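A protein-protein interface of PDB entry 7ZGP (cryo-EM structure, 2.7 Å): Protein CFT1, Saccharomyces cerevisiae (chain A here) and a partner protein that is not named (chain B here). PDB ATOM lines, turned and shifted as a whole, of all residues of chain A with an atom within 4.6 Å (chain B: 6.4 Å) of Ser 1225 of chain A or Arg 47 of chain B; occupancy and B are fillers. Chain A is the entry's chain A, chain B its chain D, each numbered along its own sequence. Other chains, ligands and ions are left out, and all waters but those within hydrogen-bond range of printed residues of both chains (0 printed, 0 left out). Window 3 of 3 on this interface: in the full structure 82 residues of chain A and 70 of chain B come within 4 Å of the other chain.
O of Ser 1225 of chain A sits close to NE of Arg 47 of chain B, at 3.5 Å. The backbone carbonyl oxygen (O) of Met 1172 of chain A sits at hydrogen-bond distance from the guanidinium group (NH2) of Arg 47 of chain B, 2.6 Å away. NH2 of Arg 47 of chain B sits at hydrogen-bond distance from O of Thr 1129 of chain A (2.7 Å).
NH2 of Arg 46 of chain B sits close to OH of Tyr 43 of chain B. The backbone NH (N) of Ser 1225 of chain A sits at hydrogen-bond distance from the backbone carbonyl oxygen (O) of Gly 1249 of chain A, at 2.9 Å. OG of Ser 1225 of chain A lies within hydrogen-bond range of SG of Cys 1226 of chain A, 3.6 Å away. The backbone carbonyl oxygen (O) of Thr 1223 of chain A is in hydrogen-bond range of the backbone NH (N) of Val 1251 of chain A.
O of Arg 47 of chain B touches CG2 of Thr 512 of chain A (3.4 Å). Thr 512 of chain A touches His 48 of chain B (CG2 to ND1, 3.4 Å). Tyr 43 of chain B touches Thr 1129 of chain A. Met 1172 of chain A touches Tyr 43 of chain B. Met 1172 of chain A touches Arg 46 of chain B. Thr 1223 of chain A touches Arg 46 of chain B (OG1 to O, 3.97 Å). Val 1251 of chain A touches Arg 46 of chain B (CG2 to O, 3.6 Å). Arg 47 of chain B touches Val 1251 of chain A. Val 1251 of chain A touches Gly 49 of chain B.
Of chain B, only Arg 47 (3.3 Å) comes within 4 Å of Ser 1225 of chain A. Of the printed residues of chain A, Arg 47 of chain B touches Thr 512 (3.4 Å), Thr 1129 (2.7 Å), Met 1172 (2.6 Å), Ser 1225 (3.3 Å) and Val 1251 (3.6 Å). Of the printed residues of chain B, Thr 1129 of chain A touches Tyr 43 (3.3 Å) and Arg 47 (2.7 Å). Printed residues of chain A within 4 Å of Tyr 43 of chain B: Thr 1129 (3.3 Å) and Met 1172 (3.5 Å). Asn 1224 of chain A touches none of the printed residues of chain B. The nearest residue of chain B that does not touch Ser 1225 of chain A is His 48 of chain B (5.4 Å). The nearest printed residue of chain A that does not touch His 48 of chain B is Val 1251 of chain A (4.4 Å).
Printed residues of chain A that touch a printed residue of chain B: Thr 512, Thr 1129, Met 1172, Thr 1223, Ser 1225 and Val 1251. Along chain A the printed residues that touch a printed residue of chain B span positions 512 to 1251. Hydrophobic or aromatic side chains of chain B within 4 Å of the printed part of chain A: Tyr 43 and His 48. Among the printed residues, 12 pairs touch across the chains. Among the printed residues, no Asp or Glu carboxylate lies within 4 Å of a Lys or Arg side-chain nitrogen of the other chain.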
ATOM      1  N   ILE A 511     -24.039 -22.383 -19.530  1.00  0.00           N
ATOM      2  CA  ILE A 511     -23.666 -22.132 -18.108  1.00  0.00           C
ATOM      3  C   ILE A 511     -22.241 -21.587 -18.137  1.00  0.00           C
ATOM      4  O   ILE A 511     -21.320 -22.392 -18.329  1.00  0.00           O
ATOM      5  CB  ILE A 511     -23.797 -23.415 -17.268  1.00  0.00           C
ATOM      6  CG1 ILE A 511     -25.245 -23.912 -17.247  1.00  0.00           C
ATOM      7  CG2 ILE A 511     -23.250 -23.201 -15.866  1.00  0.00           C
ATOM      8  CD1 ILE A 511     -25.422 -25.265 -16.607  1.00  0.00           C
ATOM      9  N   THR A 512     -22.075 -20.272 -17.977  1.00  0.00           N
ATOM     10  CA  THR A 512     -20.731 -19.657 -18.127  1.00  0.00           C
ATOM     11  C   THR A 512     -20.085 -19.410 -16.760  1.00  0.00           C
ATOM     12  O   THR A 512     -18.900 -19.032 -16.735  1.00  0.00           O
ATOM     13  CB  THR A 512     -20.839 -18.363 -18.942  1.00  0.00           C
ATOM     14  OG1 THR A 512     -21.714 -17.477 -18.244  1.00  0.00           O
ATOM     15  CG2 THR A 512     -21.360 -18.596 -20.343  1.00  0.00           C
ATOM     16  N   THR A1129      -5.483 -19.107 -18.678  1.00  0.00           N
ATOM     17  CA  THR A1129      -6.895 -19.385 -18.910  1.00  0.00           C
ATOM     18  C   THR A1129      -7.673 -19.602 -17.621  1.00  0.00           C
ATOM     19  O   THR A1129      -8.817 -19.155 -17.511  1.00  0.00           O
ATOM     20  CB  THR A1129      -7.047 -20.618 -19.803  1.00  0.00           C
ATOM     21  OG1 THR A1129      -6.783 -21.797 -19.036  1.00  0.00           O
ATOM     22  CG2 THR A1129      -6.064 -20.552 -20.947  1.00  0.00           C
ATOM     23  N   ASP A1130      -7.074 -20.281 -16.646  1.00  0.00           N
ATOM     24  CA  ASP A1130      -7.706 -20.505 -15.357  1.00  0.00           C
ATOM     25  C   ASP A1130      -6.618 -20.664 -14.310  1.00  0.00           C
ATOM     26  O   ASP A1130      -5.465 -20.967 -14.624  1.00  0.00           O
ATOM     27  CB  ASP A1130      -8.618 -21.736 -15.376  1.00  0.00           C
ATOM     28  CG  ASP A1130      -9.711 -21.668 -14.327  1.00  0.00           C
ATOM     29  OD1 ASP A1130      -9.831 -20.620 -13.659  1.00  0.00           O
ATOM     30  OD2 ASP A1130     -10.447 -22.663 -14.166  1.00  0.00           O
ATOM     31  N   MET A1172      -9.054 -25.205 -20.659  1.00  0.00           N
ATOM     32  CA  MET A1172     -10.169 -24.297 -20.434  1.00  0.00           C
ATOM     33  C   MET A1172     -10.340 -23.974 -18.957  1.00  0.00           C
ATOM     34  O   MET A1172     -10.341 -22.801 -18.574  1.00  0.00           O
ATOM     35  CB  MET A1172     -11.460 -24.896 -21.007  1.00  0.00           C
ATOM     36  CG  MET A1172     -11.405 -25.173 -22.501  1.00  0.00           C
ATOM     37  SD  MET A1172     -11.468 -23.674 -23.496  1.00  0.00           S
ATOM     38  CE  MET A1172     -12.929 -22.885 -22.828  1.00  0.00           C
ATOM     39  N   SER A1173     -10.478 -24.991 -18.109  1.00  0.00           N
ATOM     40  CA  SER A1173     -10.645 -24.789 -16.679  1.00  0.00           C
ATOM     41  C   SER A1173      -9.753 -25.761 -15.922  1.00  0.00           C
ATOM     42  O   SER A1173      -9.363 -26.812 -16.437  1.00  0.00           O
ATOM     43  CB  SER A1173     -12.104 -24.970 -16.246  1.00  0.00           C
ATOM     44  OG  SER A1173     -12.897 -23.870 -16.654  1.00  0.00           O
ATOM     45  N   THR A1223     -18.033 -28.355 -24.604  1.00  0.00           N
ATOM     46  CA  THR A1223     -16.914 -27.593 -24.069  1.00  0.00           C
ATOM     47  C   THR A1223     -17.233 -27.068 -22.676  1.00  0.00           C
ATOM     48  O   THR A1223     -18.343 -26.602 -22.406  1.00  0.00           O
ATOM     49  CB  THR A1223     -16.556 -26.439 -25.005  1.00  0.00           C
ATOM     50  OG1 THR A1223     -15.732 -25.492 -24.314  1.00  0.00           O
ATOM     51  CG2 THR A1223     -17.808 -25.753 -25.518  1.00  0.00           C
ATOM     52  N   ASN A1224     -16.247 -27.146 -21.788  1.00  0.00           N
ATOM     53  CA  ASN A1224     -16.417 -26.761 -20.396  1.00  0.00           C
ATOM     54  C   ASN A1224     -16.100 -25.283 -20.224  1.00  0.00           C
ATOM     55  O   ASN A1224     -15.067 -24.803 -20.700  1.00  0.00           O
ATOM     56  CB  ASN A1224     -15.519 -27.608 -19.496  1.00  0.00           C
ATOM     57  CG  ASN A1224     -15.517 -27.137 -18.061  1.00  0.00           C
ATOM     58  OD1 ASN A1224     -14.473 -26.795 -17.510  1.00  0.00           O
ATOM     59  ND2 ASN A1224     -16.690 -27.122 -17.440  1.00  0.00           N
ATOM     60  N   SER A1225     -17.008 -24.565 -19.563  1.00  0.00           N
ATOM     61  CA  SER A1225     -16.831 -23.104 -19.380  1.00  0.00           C
ATOM     62  C   SER A1225     -16.270 -22.814 -17.989  1.00  0.00           C
ATOM     63  O   SER A1225     -15.581 -21.790 -17.840  1.00  0.00           O
ATOM     64  CB  SER A1225     -18.136 -22.398 -19.571  1.00  0.00           C
ATOM     65  OG  SER A1225     -19.051 -22.784 -18.561  1.00  0.00           O
ATOM     66  N   CYS A1226     -16.556 -23.674 -17.009  1.00  0.00           N
ATOM     67  CA  CYS A1226     -16.122 -23.350 -15.625  1.00  0.00           C
ATOM     68  C   CYS A1226     -16.028 -24.592 -14.742  1.00  0.00           C
ATOM     69  O   CYS A1226     -16.767 -25.556 -15.002  1.00  0.00           O
ATOM     70  CB  CYS A1226     -17.108 -22.385 -14.979  1.00  0.00           C
ATOM     71  SG  CYS A1226     -18.820 -22.978 -14.999  1.00  0.00           S
ATOM     72  N   GLY A1249     -19.455 -26.441 -15.196  1.00  0.00           N
ATOM     73  CA  GLY A1249     -20.552 -25.982 -16.069  1.00  0.00           C
ATOM     74  C   GLY A1249     -20.202 -26.162 -17.533  1.00  0.00           C
ATOM     75  O   GLY A1249     -19.047 -25.892 -17.898  1.00  0.00           O
ATOM     76  N   GLN A1250     -21.166 -26.600 -18.344  1.00  0.00           N
ATOM     77  CA  GLN A1250     -20.910 -26.858 -19.784  1.00  0.00           C
ATOM     78  C   GLN A1250     -21.633 -25.805 -20.625  1.00  0.00           C
ATOM     79  O   GLN A1250     -22.576 -25.180 -20.108  1.00  0.00           O
ATOM     80  CB  GLN A1250     -21.384 -28.259 -20.167  1.00  0.00           C
ATOM     81  CG  GLN A1250     -20.698 -29.377 -19.399  1.00  0.00           C
ATOM     82  CD  GLN A1250     -19.322 -29.671 -19.940  1.00  0.00           C
ATOM     83  OE1 GLN A1250     -18.357 -28.972 -19.644  1.00  0.00           O
ATOM     84  NE2 GLN A1250     -19.223 -30.718 -20.740  1.00  0.00           N
ATOM     85  N   VAL A1251     -21.206 -25.627 -21.877  1.00  0.00           N
ATOM     86  CA  VAL A1251     -21.829 -24.614 -22.778  1.00  0.00           C
ATOM     87  C   VAL A1251     -23.217 -25.102 -23.211  1.00  0.00           C
ATOM     88  O   VAL A1251     -24.105 -24.251 -23.393  1.00  0.00           O
ATOM     89  CB  VAL A1251     -20.922 -24.317 -23.988  1.00  0.00           C
ATOM     90  CG1 VAL A1251     -21.686 -23.666 -25.129  1.00  0.00           C
ATOM     91  CG2 VAL A1251     -19.717 -23.477 -23.594  1.00  0.00           C
ATOM     92  N   ILE B  40      -8.066 -13.348 -24.797  1.00  0.00           N
ATOM     93  CA  ILE B  40      -9.218 -12.975 -23.978  1.00  0.00           C
ATOM     94  C   ILE B  40     -10.500 -13.109 -24.786  1.00  0.00           C
ATOM     95  O   ILE B  40     -11.479 -13.720 -24.343  1.00  0.00           O
ATOM     96  CB  ILE B  40      -9.049 -11.546 -23.432  1.00  0.00           C
ATOM     97  CG1 ILE B  40      -7.913 -11.484 -22.410  1.00  0.00           C
ATOM     98  CG2 ILE B  40     -10.350 -11.048 -22.827  1.00  0.00           C
ATOM     99  CD1 ILE B  40      -8.287 -12.022 -21.055  1.00  0.00           C
ATOM    100  N   LEU B  42     -11.001 -14.844 -27.580  1.00  0.00           N
ATOM    101  CA  LEU B  42     -11.232 -16.225 -27.986  1.00  0.00           C
ATOM    102  C   LEU B  42     -11.810 -17.049 -26.846  1.00  0.00           C
ATOM    103  O   LEU B  42     -12.742 -17.834 -27.050  1.00  0.00           O
ATOM    104  CB  LEU B  42      -9.930 -16.851 -28.482  1.00  0.00           C
ATOM    105  CG  LEU B  42      -9.973 -18.373 -28.611  1.00  0.00           C
ATOM    106  CD1 LEU B  42     -10.794 -18.777 -29.820  1.00  0.00           C
ATOM    107  CD2 LEU B  42      -8.576 -18.961 -28.673  1.00  0.00           C
ATOM    108  N   TYR B  43     -11.274 -16.887 -25.636  1.00  0.00           N
ATOM    109  CA  TYR B  43     -11.771 -17.673 -24.515  1.00  0.00           C
ATOM    110  C   TYR B  43     -13.136 -17.188 -24.055  1.00  0.00           C
ATOM    111  O   TYR B  43     -13.941 -17.990 -23.571  1.00  0.00           O
ATOM    112  CB  TYR B  43     -10.760 -17.655 -23.372  1.00  0.00           C
ATOM    113  CG  TYR B  43      -9.775 -18.790 -23.479  1.00  0.00           C
ATOM    114  CD1 TYR B  43     -10.054 -20.030 -22.925  1.00  0.00           C
ATOM    115  CD2 TYR B  43      -8.581 -18.635 -24.165  1.00  0.00           C
ATOM    116  CE1 TYR B  43      -9.163 -21.074 -23.033  1.00  0.00           C
ATOM    117  CE2 TYR B  43      -7.685 -19.674 -24.278  1.00  0.00           C
ATOM    118  CZ  TYR B  43      -7.982 -20.893 -23.712  1.00  0.00           C
ATOM    119  OH  TYR B  43      -7.091 -21.934 -23.820  1.00  0.00           O
ATOM    120  N   TYR B  44     -13.425 -15.894 -24.208  1.00  0.00           N
ATOM    121  CA  TYR B  44     -14.787 -15.427 -23.983  1.00  0.00           C
ATOM    122  C   TYR B  44     -15.754 -16.094 -24.950  1.00  0.00           C
ATOM    123  O   TYR B  44     -16.848 -16.512 -24.557  1.00  0.00           O
ATOM    124  CB  TYR B  44     -14.851 -13.905 -24.117  1.00  0.00           C
ATOM    125  CG  TYR B  44     -16.225 -13.327 -23.875  1.00  0.00           C
ATOM    126  CD1 TYR B  44     -17.149 -13.221 -24.907  1.00  0.00           C
ATOM    127  CD2 TYR B  44     -16.603 -12.894 -22.614  1.00  0.00           C
ATOM    128  CE1 TYR B  44     -18.404 -12.701 -24.690  1.00  0.00           C
ATOM    129  CE2 TYR B  44     -17.858 -12.371 -22.388  1.00  0.00           C
ATOM    130  CZ  TYR B  44     -18.753 -12.276 -23.429  1.00  0.00           C
ATOM    131  OH  TYR B  44     -20.004 -11.753 -23.211  1.00  0.00           O
ATOM    132  N   ASN B  45     -15.369 -16.196 -26.224  1.00  0.00           N
ATOM    133  CA  ASN B  45     -16.236 -16.851 -27.199  1.00  0.00           C
ATOM    134  C   ASN B  45     -16.414 -18.332 -26.885  1.00  0.00           C
ATOM    135  O   ASN B  45     -17.528 -18.860 -26.972  1.00  0.00           O
ATOM    136  CB  ASN B  45     -15.675 -16.668 -28.608  1.00  0.00           C
ATOM    137  CG  ASN B  45     -15.958 -15.295 -29.171  1.00  0.00           C
ATOM    138  OD1 ASN B  45     -16.771 -14.547 -28.632  1.00  0.00           O
ATOM    139  ND2 ASN B  45     -15.295 -14.957 -30.266  1.00  0.00           N
ATOM    140  N   ARG B  46     -15.329 -19.018 -26.521  1.00  0.00           N
ATOM    141  CA  ARG B  46     -15.408 -20.459 -26.300  1.00  0.00           C
ATOM    142  C   ARG B  46     -16.173 -20.792 -25.025  1.00  0.00           C
ATOM    143  O   ARG B  46     -16.931 -21.767 -24.989  1.00  0.00           O
ATOM    144  CB  ARG B  46     -14.003 -21.063 -26.267  1.00  0.00           C
ATOM    145  CG  ARG B  46     -13.242 -20.889 -27.569  1.00  0.00           C
ATOM    146  CD  ARG B  46     -12.278 -22.030 -27.834  1.00  0.00           C
ATOM    147  NE  ARG B  46     -11.072 -21.941 -27.022  1.00  0.00           N
ATOM    148  CZ  ARG B  46      -9.868 -22.317 -27.430  1.00  0.00           C
ATOM    149  NH1 ARG B  46      -9.668 -22.787 -28.649  1.00  0.00           N
ATOM    150  NH2 ARG B  46      -8.837 -22.211 -26.597  1.00  0.00           N
ATOM    151  N   ARG B  47     -15.997 -19.993 -23.970  1.00  0.00           N
ATOM    152  CA  ARG B  47     -16.708 -20.255 -22.724  1.00  0.00           C
ATOM    153  C   ARG B  47     -18.182 -19.884 -22.807  1.00  0.00           C
ATOM    154  O   ARG B  47     -18.976 -20.372 -21.997  1.00  0.00           O
ATOM    155  CB  ARG B  47     -16.049 -19.500 -21.571  1.00  0.00           C
ATOM    156  CG  ARG B  47     -14.695 -20.056 -21.172  1.00  0.00           C
ATOM    157  CD  ARG B  47     -14.177 -19.400 -19.907  1.00  0.00           C
ATOM    158  NE  ARG B  47     -12.983 -20.068 -19.408  1.00  0.00           N
ATOM    159  CZ  ARG B  47     -11.758 -19.566 -19.478  1.00  0.00           C
ATOM    160  NH1 ARG B  47     -11.528 -18.377 -20.012  1.00  0.00           N
ATOM    161  NH2 ARG B  47     -10.739 -20.272 -19.000  1.00  0.00           N
ATOM    162  N   HIS B  48     -18.563 -19.038 -23.758  1.00  0.00           N
ATOM    163  CA  HIS B  48     -19.952 -18.644 -23.935  1.00  0.00           C
ATOM    164  C   HIS B  48     -20.627 -19.356 -25.097  1.00  0.00           C
ATOM    165  O   HIS B  48     -21.789 -19.066 -25.392  1.00  0.00           O
ATOM    166  CB  HIS B  48     -20.042 -17.129 -24.135  1.00  0.00           C
ATOM    167  CG  HIS B  48     -19.864 -16.342 -22.875  1.00  0.00           C
ATOM    168  ND1 HIS B  48     -20.922 -15.790 -22.186  1.00  0.00           N
ATOM    169  CD2 HIS B  48     -18.751 -16.020 -22.175  1.00  0.00           C
ATOM    170  CE1 HIS B  48     -20.468 -15.159 -21.119  1.00  0.00           C
ATOM    171  NE2 HIS B  48     -19.153 -15.284 -21.088  1.00  0.00           N
ATOM    172  N   GLY B  49     -19.933 -20.277 -25.762  1.00  0.00           N
ATOM    173  CA  GLY B  49     -20.508 -20.964 -26.898  1.00  0.00           C
ATOM    174  C   GLY B  49     -20.641 -20.127 -28.147  1.00  0.00           C
ATOM    175  O   GLY B  49     -21.298 -20.558 -29.098  1.00  0.00           O
ATOM    176  N   LEU B  50     -20.041 -18.945 -28.173  1.00  0.00           N
ATOM    177  CA  LEU B  50     -20.156 -18.062 -29.325  1.00  0.00           C
ATOM    178  C   LEU B  50     -19.151 -18.468 -30.398  1.00  0.00           C
ATOM    179  O   LEU B  50     -17.981 -18.704 -30.082  1.00  0.00           O
ATOM    180  CB  LEU B  50     -19.924 -16.614 -28.913  1.00  0.00           C
ATOM    181  CG  LEU B  50     -20.822 -16.087 -27.795  1.00  0.00           C
ATOM    182  CD1 LEU B  50     -20.293 -14.768 -27.262  1.00  0.00           C
ATOM    183  CD2 LEU B  50     -22.248 -15.934 -28.290  1.00  0.00           C
